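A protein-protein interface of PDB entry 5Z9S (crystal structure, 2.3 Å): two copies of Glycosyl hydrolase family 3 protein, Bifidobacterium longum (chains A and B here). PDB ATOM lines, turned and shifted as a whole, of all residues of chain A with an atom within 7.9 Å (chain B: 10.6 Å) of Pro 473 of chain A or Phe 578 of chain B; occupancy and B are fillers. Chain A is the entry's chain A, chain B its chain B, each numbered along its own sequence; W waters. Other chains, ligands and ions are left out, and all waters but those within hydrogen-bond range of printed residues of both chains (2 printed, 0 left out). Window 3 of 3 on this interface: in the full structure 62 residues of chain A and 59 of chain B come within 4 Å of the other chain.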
ATOM      1  N   VAL A 470      25.980  27.720  19.352  1.00  0.00           N
ATOM      2  CA  VAL A 470      26.811  27.961  18.176  1.00  0.00           C
ATOM      3  C   VAL A 470      25.977  28.707  17.144  1.00  0.00           C
ATOM      4  O   VAL A 470      24.748  28.550  17.111  1.00  0.00           O
ATOM      5  CB  VAL A 470      27.374  26.651  17.598  1.00  0.00           C
ATOM      6  CG1 VAL A 470      28.206  25.924  18.643  1.00  0.00           C
ATOM      7  CG2 VAL A 470      26.255  25.765  17.078  1.00  0.00           C
ATOM      8  N   PRO A 471      26.589  29.545  16.309  1.00  0.00           N
ATOM      9  CA  PRO A 471      25.822  30.246  15.277  1.00  0.00           C
ATOM     10  C   PRO A 471      25.147  29.278  14.317  1.00  0.00           C
ATOM     11  O   PRO A 471      25.667  28.202  14.014  1.00  0.00           O
ATOM     12  CB  PRO A 471      26.883  31.091  14.561  1.00  0.00           C
ATOM     13  CG  PRO A 471      27.967  31.266  15.573  1.00  0.00           C
ATOM     14  CD  PRO A 471      27.996  29.980  16.347  1.00  0.00           C
ATOM     15  N   ASP A 472      23.964  29.668  13.860  1.00  0.00           N
ATOM     16  CA  ASP A 472      23.217  28.864  12.905  1.00  0.00           C
ATOM     17  C   ASP A 472      24.017  28.762  11.612  1.00  0.00           C
ATOM     18  O   ASP A 472      24.332  29.797  11.006  1.00  0.00           O
ATOM     19  CB  ASP A 472      21.846  29.483  12.643  1.00  0.00           C
ATOM     20  CG  ASP A 472      20.891  28.529  11.946  1.00  0.00           C
ATOM     21  OD1 ASP A 472      21.293  27.879  10.958  1.00  0.00           O
ATOM     22  OD2 ASP A 472      19.731  28.424  12.395  1.00  0.00           O
ATOM     23  N   PRO A 473      24.361  27.554  11.155  1.00  0.00           N
ATOM     24  CA  PRO A 473      25.257  27.426   9.994  1.00  0.00           C
ATOM     25  C   PRO A 473      24.692  28.009   8.710  1.00  0.00           C
ATOM     26  O   PRO A 473      25.458  28.208   7.759  1.00  0.00           O
ATOM     27  CB  PRO A 473      25.458  25.908   9.867  1.00  0.00           C
ATOM     28  CG  PRO A 473      25.063  25.346  11.196  1.00  0.00           C
ATOM     29  CD  PRO A 473      23.981  26.243  11.705  1.00  0.00           C
ATOM     30  N   ALA A 474      23.393  28.283   8.647  1.00  0.00           N
ATOM     31  CA  ALA A 474      22.774  28.844   7.448  1.00  0.00           C
ATOM     32  C   ALA A 474      22.691  30.360   7.489  1.00  0.00           C
ATOM     33  O   ALA A 474      21.696  30.935   7.039  1.00  0.00           O
ATOM     34  CB  ALA A 474      21.391  28.234   7.254  1.00  0.00           C
ATOM     35  N   GLY A 475      23.700  31.041   8.002  1.00  0.00           N
ATOM     36  CA  GLY A 475      23.594  32.485   8.000  1.00  0.00           C
ATOM     37  C   GLY A 475      23.310  33.038   9.388  1.00  0.00           C
ATOM     38  O   GLY A 475      22.717  32.374  10.247  1.00  0.00           O
ATOM     39  N   GLU A 476      23.756  34.273   9.616  1.00  0.00           N
ATOM     40  CA  GLU A 476      23.515  34.928  10.894  1.00  0.00           C
ATOM     41  C   GLU A 476      22.159  35.610  10.948  1.00  0.00           C
ATOM     42  O   GLU A 476      21.709  35.976  12.040  1.00  0.00           O
ATOM     43  CB  GLU A 476      24.581  35.994  11.173  1.00  0.00           C
ATOM     44  CG  GLU A 476      26.008  35.585  10.911  1.00  0.00           C
ATOM     45  CD  GLU A 476      26.979  36.716  11.195  1.00  0.00           C
ATOM     46  OE1 GLU A 476      27.823  37.007  10.320  1.00  0.00           O
ATOM     47  OE2 GLU A 476      26.900  37.312  12.290  1.00  0.00           O
ATOM     48  N   ARG A 484      19.247  35.003  13.159  1.00  0.00           N
ATOM     49  CA  ARG A 484      18.936  33.611  13.450  1.00  0.00           C
ATOM     50  C   ARG A 484      19.454  33.261  14.841  1.00  0.00           C
ATOM     51  O   ARG A 484      20.639  33.476  15.126  1.00  0.00           O
ATOM     52  CB  ARG A 484      19.558  32.682  12.405  1.00  0.00           C
ATOM     53  CG  ARG A 484      19.018  32.860  10.991  1.00  0.00           C
ATOM     54  CD  ARG A 484      19.642  31.851  10.039  1.00  0.00           C
ATOM     55  NE  ARG A 484      19.370  32.160   8.638  1.00  0.00           N
ATOM     56  CZ  ARG A 484      18.461  31.538   7.894  1.00  0.00           C
ATOM     57  NH1 ARG A 484      17.726  30.564   8.412  1.00  0.00           N
ATOM     58  NH2 ARG A 484      18.287  31.889   6.628  1.00  0.00           N
ATOM     59  N   PRO A 485      18.607  32.750  15.732  1.00  0.00           N
ATOM     60  CA  PRO A 485      19.077  32.404  17.079  1.00  0.00           C
ATOM     61  C   PRO A 485      20.159  31.337  17.023  1.00  0.00           C
ATOM     62  O   PRO A 485      20.219  30.529  16.095  1.00  0.00           O
ATOM     63  CB  PRO A 485      17.819  31.871  17.775  1.00  0.00           C
ATOM     64  CG  PRO A 485      16.669  32.396  16.990  1.00  0.00           C
ATOM     65  CD  PRO A 485      17.144  32.648  15.591  1.00  0.00           C
ATOM     66  N   LYS A 486      21.020  31.336  18.035  1.00  0.00           N
ATOM     67  CA  LYS A 486      22.043  30.305  18.102  1.00  0.00           C
ATOM     68  C   LYS A 486      21.401  28.956  18.401  1.00  0.00           C
ATOM     69  O   LYS A 486      20.334  28.869  19.013  1.00  0.00           O
ATOM     70  CB  LYS A 486      23.093  30.651  19.157  1.00  0.00           C
ATOM     71  CG  LYS A 486      23.845  31.937  18.858  1.00  0.00           C
ATOM     72  CD  LYS A 486      24.994  32.162  19.830  1.00  0.00           C
ATOM     73  CE  LYS A 486      25.832  33.358  19.412  1.00  0.00           C
ATOM     74  NZ  LYS A 486      24.992  34.569  19.191  1.00  0.00           N
ATOM     75  N   ILE A 487      22.065  27.897  17.953  1.00  0.00           N
ATOM     76  CA  ILE A 487      21.598  26.530  18.136  1.00  0.00           C
ATOM     77  C   ILE A 487      22.402  25.879  19.251  1.00  0.00           C
ATOM     78  O   ILE A 487      23.635  25.990  19.289  1.00  0.00           O
ATOM     79  CB  ILE A 487      21.712  25.722  16.831  1.00  0.00           C
ATOM     80  CG1 ILE A 487      20.958  26.428  15.702  1.00  0.00           C
ATOM     81  CG2 ILE A 487      21.170  24.313  17.028  1.00  0.00           C
ATOM     82  CD1 ILE A 487      19.495  26.657  16.003  1.00  0.00           C
ATOM     83  N   GLY A 488      21.705  25.223  20.177  1.00  0.00           N
ATOM     84  CA  GLY A 488      22.383  24.511  21.242  1.00  0.00           C
ATOM     85  C   GLY A 488      22.860  23.164  20.741  1.00  0.00           C
ATOM     86  O   GLY A 488      22.093  22.398  20.147  1.00  0.00           O
ATOM     87  N   VAL A 489      24.137  22.877  20.967  1.00  0.00           N
ATOM     88  CA  VAL A 489      24.730  21.587  20.644  1.00  0.00           C
ATOM     89  C   VAL A 489      25.299  21.007  21.928  1.00  0.00           C
ATOM     90  O   VAL A 489      25.448  21.702  22.934  1.00  0.00           O
ATOM     91  CB  VAL A 489      25.818  21.688  19.556  1.00  0.00           C
ATOM     92  CG1 VAL A 489      25.269  22.389  18.323  1.00  0.00           C
ATOM     93  CG2 VAL A 489      27.049  22.402  20.092  1.00  0.00           C
ATOM     94  N   SER A 490      25.593  19.710  21.894  1.00  0.00           N
ATOM     95  CA  SER A 490      26.168  19.057  23.062  1.00  0.00           C
ATOM     96  C   SER A 490      27.432  19.794  23.476  1.00  0.00           C
ATOM     97  O   SER A 490      28.382  19.903  22.695  1.00  0.00           O
ATOM     98  CB  SER A 490      26.476  17.595  22.757  1.00  0.00           C
ATOM     99  OG  SER A 490      27.008  16.951  23.900  1.00  0.00           O
ATOM    100  N   VAL B 572      34.180   7.812  10.988  1.00  0.00           N
ATOM    101  CA  VAL B 572      33.082   8.489  10.303  1.00  0.00           C
ATOM    102  C   VAL B 572      32.914   9.938  10.740  1.00  0.00           C
ATOM    103  O   VAL B 572      32.092  10.656  10.149  1.00  0.00           O
ATOM    104  CB  VAL B 572      31.747   7.734  10.493  1.00  0.00           C
ATOM    105  CG1 VAL B 572      31.823   6.350   9.864  1.00  0.00           C
ATOM    106  CG2 VAL B 572      31.379   7.646  11.968  1.00  0.00           C
ATOM    107  N   GLY B 573      33.663  10.390  11.735  1.00  0.00           N
ATOM    108  CA  GLY B 573      33.495  11.720  12.280  1.00  0.00           C
ATOM    109  C   GLY B 573      32.467  11.755  13.397  1.00  0.00           C
ATOM    110  O   GLY B 573      31.582  10.908  13.502  1.00  0.00           O
ATOM    111  N   GLU B 574      32.602  12.765  14.252  1.00  0.00           N
ATOM    112  CA  GLU B 574      31.687  12.928  15.373  1.00  0.00           C
ATOM    113  C   GLU B 574      30.290  13.262  14.878  1.00  0.00           C
ATOM    114  O   GLU B 574      30.121  14.043  13.938  1.00  0.00           O
ATOM    115  CB  GLU B 574      32.172  14.045  16.298  1.00  0.00           C
ATOM    116  CG  GLU B 574      33.472  13.760  17.022  1.00  0.00           C
ATOM    117  CD  GLU B 574      33.248  13.446  18.483  1.00  0.00           C
ATOM    118  OE1 GLU B 574      33.104  12.251  18.818  1.00  0.00           O
ATOM    119  OE2 GLU B 574      33.189  14.396  19.293  1.00  0.00           O
ATOM    120  N   TYR B 575      29.282  12.685  15.519  1.00  0.00           N
ATOM    121  CA  TYR B 575      27.914  13.026  15.173  1.00  0.00           C
ATOM    122  C   TYR B 575      27.406  14.070  16.156  1.00  0.00           C
ATOM    123  O   TYR B 575      27.973  14.271  17.233  1.00  0.00           O
ATOM    124  CB  TYR B 575      26.988  11.797  15.153  1.00  0.00           C
ATOM    125  CG  TYR B 575      26.873  10.976  16.428  1.00  0.00           C
ATOM    126  CD1 TYR B 575      26.419  11.539  17.616  1.00  0.00           C
ATOM    127  CD2 TYR B 575      27.179   9.623  16.427  1.00  0.00           C
ATOM    128  CE1 TYR B 575      26.302  10.787  18.766  1.00  0.00           C
ATOM    129  CE2 TYR B 575      27.063   8.865  17.574  1.00  0.00           C
ATOM    130  CZ  TYR B 575      26.625   9.453  18.739  1.00  0.00           C
ATOM    131  OH  TYR B 575      26.505   8.700  19.882  1.00  0.00           O
ATOM    132  N   GLY B 576      26.335  14.744  15.765  1.00  0.00           N
ATOM    133  CA  GLY B 576      25.780  15.785  16.603  1.00  0.00           C
ATOM    134  C   GLY B 576      24.629  16.457  15.896  1.00  0.00           C
ATOM    135  O   GLY B 576      24.152  15.986  14.860  1.00  0.00           O
ATOM    136  N   VAL B 577      24.174  17.564  16.488  1.00  0.00           N
ATOM    137  CA  VAL B 577      23.165  18.394  15.836  1.00  0.00           C
ATOM    138  C   VAL B 577      23.606  18.737  14.422  1.00  0.00           C
ATOM    139  O   VAL B 577      22.805  18.719  13.481  1.00  0.00           O
ATOM    140  CB  VAL B 577      22.903  19.661  16.673  1.00  0.00           C
ATOM    141  CG1 VAL B 577      21.822  20.521  16.033  1.00  0.00           C
ATOM    142  CG2 VAL B 577      22.533  19.281  18.097  1.00  0.00           C
ATOM    143  N   PHE B 578      24.888  19.048  14.253  1.00  0.00           N
ATOM    144  CA  PHE B 578      25.520  19.179  12.949  1.00  0.00           C
ATOM    145  C   PHE B 578      26.719  18.242  12.874  1.00  0.00           C
ATOM    146  O   PHE B 578      27.423  18.039  13.868  1.00  0.00           O
ATOM    147  CB  PHE B 578      25.946  20.621  12.680  1.00  0.00           C
ATOM    148  CG  PHE B 578      24.856  21.620  12.926  1.00  0.00           C
ATOM    149  CD1 PHE B 578      23.766  21.692  12.075  1.00  0.00           C
ATOM    150  CD2 PHE B 578      24.910  22.472  14.016  1.00  0.00           C
ATOM    151  CE1 PHE B 578      22.756  22.603  12.298  1.00  0.00           C
ATOM    152  CE2 PHE B 578      23.901  23.388  14.248  1.00  0.00           C
ATOM    153  CZ  PHE B 578      22.822  23.453  13.389  1.00  0.00           C
ATOM    154  N   ALA B 579      26.931  17.657  11.698  1.00  0.00           N
ATOM    155  CA  ALA B 579      28.023  16.721  11.490  1.00  0.00           C
ATOM    156  C   ALA B 579      28.440  16.778  10.030  1.00  0.00           C
ATOM    157  O   ALA B 579      27.645  17.134   9.158  1.00  0.00           O
ATOM    158  CB  ALA B 579      27.631  15.291  11.881  1.00  0.00           C
ATOM    159  N   LYS B 580      29.693  16.424   9.774  1.00  0.00           N
ATOM    160  CA  LYS B 580      30.219  16.482   8.420  1.00  0.00           C
ATOM    161  C   LYS B 580      29.730  15.300   7.591  1.00  0.00           C
ATOM    162  O   LYS B 580      29.431  14.222   8.112  1.00  0.00           O
ATOM    163  CB  LYS B 580      31.748  16.506   8.439  1.00  0.00           C
ATOM    164  CG  LYS B 580      32.337  17.812   8.938  1.00  0.00           C
ATOM    165  CD  LYS B 580      33.819  17.667   9.235  1.00  0.00           C
ATOM    166  CE  LYS B 580      34.355  18.887   9.970  1.00  0.00           C
ATOM    167  NZ  LYS B 580      35.021  18.516  11.248  1.00  0.00           N
ATOM    168  N   ARG B 581      29.638  15.525   6.283  1.00  0.00           N
ATOM    169  CA  ARG B 581      29.321  14.461   5.342  1.00  0.00           C
ATOM    170  C   ARG B 581      30.376  13.365   5.420  1.00  0.00           C
ATOM    171  O   ARG B 581      31.565  13.617   5.201  1.00  0.00           O
ATOM    172  CB  ARG B 581      29.238  15.037   3.929  1.00  0.00           C
ATOM    173  CG  ARG B 581      29.083  14.004   2.837  1.00  0.00           C
ATOM    174  CD  ARG B 581      27.667  13.471   2.756  1.00  0.00           C
ATOM    175  NE  ARG B 581      27.557  12.472   1.698  1.00  0.00           N
ATOM    176  CZ  ARG B 581      27.241  12.749   0.438  1.00  0.00           C
ATOM    177  NH1 ARG B 581      26.982  13.998   0.075  1.00  0.00           N
ATOM    178  NH2 ARG B 581      27.177  11.775  -0.456  1.00  0.00           N
ATOM    179  N   VAL B 582      29.938  12.146   5.741  1.00  0.00           N
ATOM    180  CA  VAL B 582      30.882  11.075   6.043  1.00  0.00           C
ATOM    181  C   VAL B 582      31.685  10.673   4.811  1.00  0.00           C
ATOM    182  O   VAL B 582      32.857  10.297   4.924  1.00  0.00           O
ATOM    183  CB  VAL B 582      30.138   9.874   6.653  1.00  0.00           C
ATOM    184  CG1 VAL B 582      31.129   8.823   7.118  1.00  0.00           C
ATOM    185  CG2 VAL B 582      29.261  10.331   7.807  1.00  0.00           C
ATOM    186  N   THR B 587      36.656  13.963   5.930  1.00  0.00           N
ATOM    187  CA  THR B 587      35.978  13.542   7.144  1.00  0.00           C
ATOM    188  C   THR B 587      36.685  12.335   7.745  1.00  0.00           C
ATOM    189  O   THR B 587      37.098  11.418   7.029  1.00  0.00           O
ATOM    190  CB  THR B 587      34.517  13.210   6.845  1.00  0.00           C
ATOM    191  OG1 THR B 587      33.909  14.321   6.176  1.00  0.00           O
ATOM    192  CG2 THR B 587      33.756  12.925   8.128  1.00  0.00           C
ATOM    193  N   ARG B 626      23.508   6.913  11.455  1.00  0.00           N
ATOM    194  CA  ARG B 626      24.572   7.313  12.369  1.00  0.00           C
ATOM    195  C   ARG B 626      24.355   6.751  13.767  1.00  0.00           C
ATOM    196  O   ARG B 626      25.323   6.539  14.503  1.00  0.00           O
ATOM    197  CB  ARG B 626      24.668   8.838  12.447  1.00  0.00           C
ATOM    198  CG  ARG B 626      25.034   9.526  11.149  1.00  0.00           C
ATOM    199  CD  ARG B 626      25.065  11.027  11.354  1.00  0.00           C
ATOM    200  NE  ARG B 626      25.451  11.760  10.154  1.00  0.00           N
ATOM    201  CZ  ARG B 626      26.687  12.174   9.899  1.00  0.00           C
ATOM    202  NH1 ARG B 626      27.662  11.924  10.760  1.00  0.00           N
ATOM    203  NH2 ARG B 626      26.948  12.842   8.784  1.00  0.00           N
ATOM    204  N   GLN B 630      18.222   7.355  15.269  1.00  0.00           N
ATOM    205  CA  GLN B 630      17.895   8.033  14.024  1.00  0.00           C
ATOM    206  C   GLN B 630      16.810   7.317  13.230  1.00  0.00           C
ATOM    207  O   GLN B 630      16.234   7.916  12.315  1.00  0.00           O
ATOM    208  CB  GLN B 630      19.162   8.156  13.170  1.00  0.00           C
ATOM    209  CG  GLN B 630      19.327   9.451  12.401  1.00  0.00           C
ATOM    210  CD  GLN B 630      20.645   9.499  11.638  1.00  0.00           C
ATOM    211  OE1 GLN B 630      21.212   8.461  11.289  1.00  0.00           O
ATOM    212  NE2 GLN B 630      21.139  10.705  11.379  1.00  0.00           N
ATOM    213  N   ASP B 644      13.793  19.422  10.949  1.00  0.00           N
ATOM    214  CA  ASP B 644      14.563  18.406  10.243  1.00  0.00           C
ATOM    215  C   ASP B 644      15.767  17.914  11.038  1.00  0.00           C
ATOM    216  O   ASP B 644      16.659  17.286  10.454  1.00  0.00           O
ATOM    217  CB  ASP B 644      15.022  18.922   8.869  1.00  0.00           C
ATOM    218  CG  ASP B 644      15.976  20.098   8.965  1.00  0.00           C
ATOM    219  OD1 ASP B 644      16.151  20.658  10.069  1.00  0.00           O
ATOM    220  OD2 ASP B 644      16.549  20.471   7.921  1.00  0.00           O
ATOM    221  N   ARG B 645      15.835  18.192  12.338  1.00  0.00           N
ATOM    222  CA  ARG B 645      16.907  17.690  13.183  1.00  0.00           C
ATOM    223  C   ARG B 645      16.315  17.201  14.493  1.00  0.00           C
ATOM    224  O   ARG B 645      15.300  17.717  14.963  1.00  0.00           O
ATOM    225  CB  ARG B 645      17.974  18.756  13.496  1.00  0.00           C
ATOM    226  CG  ARG B 645      18.598  19.443  12.293  1.00  0.00           C
ATOM    227  CD  ARG B 645      19.724  20.372  12.733  1.00  0.00           C
ATOM    228  NE  ARG B 645      19.308  21.255  13.819  1.00  0.00           N
ATOM    229  CZ  ARG B 645      18.759  22.451  13.639  1.00  0.00           C
ATOM    230  NH1 ARG B 645      18.559  22.912  12.414  1.00  0.00           N
ATOM    231  NH2 ARG B 645      18.407  23.185  14.686  1.00  0.00           N
ATOM    232  N   TYR B 646      16.958  16.196  15.076  1.00  0.00           N
ATOM    233  CA  TYR B 646      16.802  15.962  16.499  1.00  0.00           C
ATOM    234  C   TYR B 646      17.618  17.002  17.254  1.00  0.00           C
ATOM    235  O   TYR B 646      18.627  17.507  16.755  1.00  0.00           O
ATOM    236  CB  TYR B 646      17.263  14.557  16.892  1.00  0.00           C
ATOM    237  CG  TYR B 646      16.445  13.422  16.320  1.00  0.00           C
ATOM    238  CD1 TYR B 646      16.732  12.897  15.069  1.00  0.00           C
ATOM    239  CD2 TYR B 646      15.401  12.858  17.042  1.00  0.00           C
ATOM    240  CE1 TYR B 646      15.995  11.851  14.547  1.00  0.00           C
ATOM    241  CE2 TYR B 646      14.658  11.811  16.528  1.00  0.00           C
ATOM    242  CZ  TYR B 646      14.959  11.312  15.278  1.00  0.00           C
ATOM    243  OH  TYR B 646      14.225  10.271  14.758  1.00  0.00           O
ATOM    244  N   ALA B 647      17.175  17.324  18.470  1.00  0.00           N
ATOM    245  CA  ALA B 647      17.877  18.331  19.255  1.00  0.00           C
ATOM    246  C   ALA B 647      19.288  17.902  19.630  1.00  0.00           C
ATOM    247  O   ALA B 647      20.083  18.749  20.050  1.00  0.00           O
ATOM    248  CB  ALA B 647      17.079  18.667  20.517  1.00  0.00           C
ATOM    249  N   ASP B 648      19.623  16.619  19.474  1.00  0.00           N
ATOM    250  CA  ASP B 648      20.940  16.112  19.818  1.00  0.00           C
ATOM    251  C   ASP B 648      21.614  15.360  18.681  1.00  0.00           C
ATOM    252  O   ASP B 648      22.703  14.813  18.886  1.00  0.00           O
ATOM    253  CB  ASP B 648      20.852  15.182  21.038  1.00  0.00           C
ATOM    254  CG  ASP B 648      20.040  13.932  20.755  1.00  0.00           C
ATOM    255  OD1 ASP B 648      19.246  13.945  19.792  1.00  0.00           O
ATOM    256  OD2 ASP B 648      20.195  12.939  21.490  1.00  0.00           O
ATOM    257  N   LEU B 649      21.006  15.299  17.500  1.00  0.00           N
ATOM    258  CA  LEU B 649      21.569  14.490  16.429  1.00  0.00           C
ATOM    259  C   LEU B 649      21.007  14.958  15.097  1.00  0.00           C
ATOM    260  O   LEU B 649      19.797  15.164  14.969  1.00  0.00           O
ATOM    261  CB  LEU B 649      21.265  13.005  16.642  1.00  0.00           C
ATOM    262  CG  LEU B 649      21.895  12.080  15.604  1.00  0.00           C
ATOM    263  CD1 LEU B 649      23.406  12.130  15.738  1.00  0.00           C
ATOM    264  CD2 LEU B 649      21.387  10.661  15.753  1.00  0.00           C
ATOM    265  N   THR B 650      21.885  15.120  14.116  1.00  0.00           N
ATOM    266  CA  THR B 650      21.441  15.439  12.770  1.00  0.00           C
ATOM    267  C   THR B 650      20.632  14.283  12.192  1.00  0.00           C
ATOM    268  O   THR B 650      20.817  13.120  12.556  1.00  0.00           O
ATOM    269  CB  THR B 650      22.643  15.732  11.872  1.00  0.00           C
ATOM    270  OG1 THR B 650      22.193  16.051  10.553  1.00  0.00           O
ATOM    271  CG2 THR B 650      23.561  14.520  11.800  1.00  0.00           C
ATOM    272  N   GLN B 651      19.710  14.613  11.296  1.00  0.00           N
ATOM    273  CA  GLN B 651      18.972  13.591  10.570  1.00  0.00           C
ATOM    274  C   GLN B 651      19.647  13.219   9.258  1.00  0.00           C
ATOM    275  O   GLN B 651      19.084  12.440   8.484  1.00  0.00           O
ATOM    276  CB  GLN B 651      17.530  14.047  10.325  1.00  0.00           C
ATOM    277  CG  GLN B 651      16.712  14.138  11.606  1.00  0.00           C
ATOM    278  CD  GLN B 651      15.241  14.441  11.360  1.00  0.00           C
ATOM    279  OE1 GLN B 651      14.717  14.206  10.270  1.00  0.00           O
ATOM    280  NE2 GLN B 651      14.572  14.973  12.377  1.00  0.00           N
ATOM    281  N   ASP B 652      20.829  13.760   8.992  1.00  0.00           N
ATOM    282  CA  ASP B 652      21.632  13.291   7.867  1.00  0.00           C
ATOM    283  C   ASP B 652      22.183  11.913   8.201  1.00  0.00           C
ATOM    284  O   ASP B 652      22.862  11.759   9.225  1.00  0.00           O
ATOM    285  CB  ASP B 652      22.778  14.266   7.567  1.00  0.00           C
ATOM    286  CG  ASP B 652      23.825  13.683   6.611  1.00  0.00           C
ATOM    287  OD1 ASP B 652      23.445  13.289   5.491  1.00  0.00           O
ATOM    288  OD2 ASP B 652      25.020  13.643   6.968  1.00  0.00           O
ATOM    289  N   PRO B 653      21.918  10.891   7.395  1.00  0.00           N
ATOM    290  CA  PRO B 653      22.490   9.574   7.670  1.00  0.00           C
ATOM    291  C   PRO B 653      23.978   9.553   7.364  1.00  0.00           C
ATOM    292  O   PRO B 653      24.515  10.435   6.695  1.00  0.00           O
ATOM    293  CB  PRO B 653      21.712   8.649   6.738  1.00  0.00           C
ATOM    294  CG  PRO B 653      21.317   9.527   5.604  1.00  0.00           C
ATOM    295  CD  PRO B 653      21.057  10.882   6.199  1.00  0.00           C
HETATM  296  O   HOH W   1      25.306  17.959  19.414  1.00  0.00           O
HETATM  297  O   HOH W   2      19.879  21.450  19.268  1.00  0.00           O
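O of Val 470 of chain A sits at hydrogen-bond distance from N of Ile 487 of chain A, at 2.9 Å. The side-chain amide nitrogen (NE2) of Gln 651 of chain B sits close to the backbone NH (N) of Arg 645 of chain B, 3.5 Å away.
Pro 473 of chain A touches Phe 578 of chain B. Ile 487 of chain A touches Val 577 of chain B (CG2 to CG1, 3.97 Å). Arg 645 of chain B touches Ile 487 of chain A. CG2 of Val 577 of chain B touches O of Gly 488 of chain A, at 3.8 Å. Val 489 of chain A touches Val 577 of chain B.
No position is printed for both chains. Of the 5 pairs that touch across the chains among the printed residues, none has its exchanged pair printed and touching as well.
Water W2 bridges O of Gly 488 of chain A and O of Ala 647 of chain B. Water W1 bridges N of Ser 490 of chain A and N of Val 577 of chain B.
No residue of chain B comes within 4 Å of Asp 472 of chain A. Pro 473 of chain A touches just one residue of chain B: Phe 578. No residue of chain B comes within 4 Å of Gly 475 of chain A. Lys 486 of chain A touches none of the printed residues of chain B. Printed residues of chain B within 4 Å of Ile 487 of chain A: Val 577 (3.97 Å) and Arg 645 (3.8 Å). Printed residues of chain B within 4 Å of Gly 488 of chain A: Val 577 (3.8 Å). Of the printed residues of chain A, Phe 578 of chain B touches Pro 473 (3.5 Å). Printed residues of chain A within 4 Å of Arg 645 of chain B: Ile 487. The nearest residue of chain B that does not touch Pro 473 of chain A is Arg 645 of chain B (6.4 Å). The nearest printed residue of chain B that does not touch Val 489 of chain A is Phe 578 of chain B (4.3 Å).
Printed residues of chain B that touch a printed residue of chain A: Val 577, Phe 578 and Arg 645. Among the printed residues, 5 pairs touch across the chains. Among the printed residues, no Asp or Glu carboxylate lies within 4 Å of a Lys or Arg side-chain nitrogen of the other chain.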
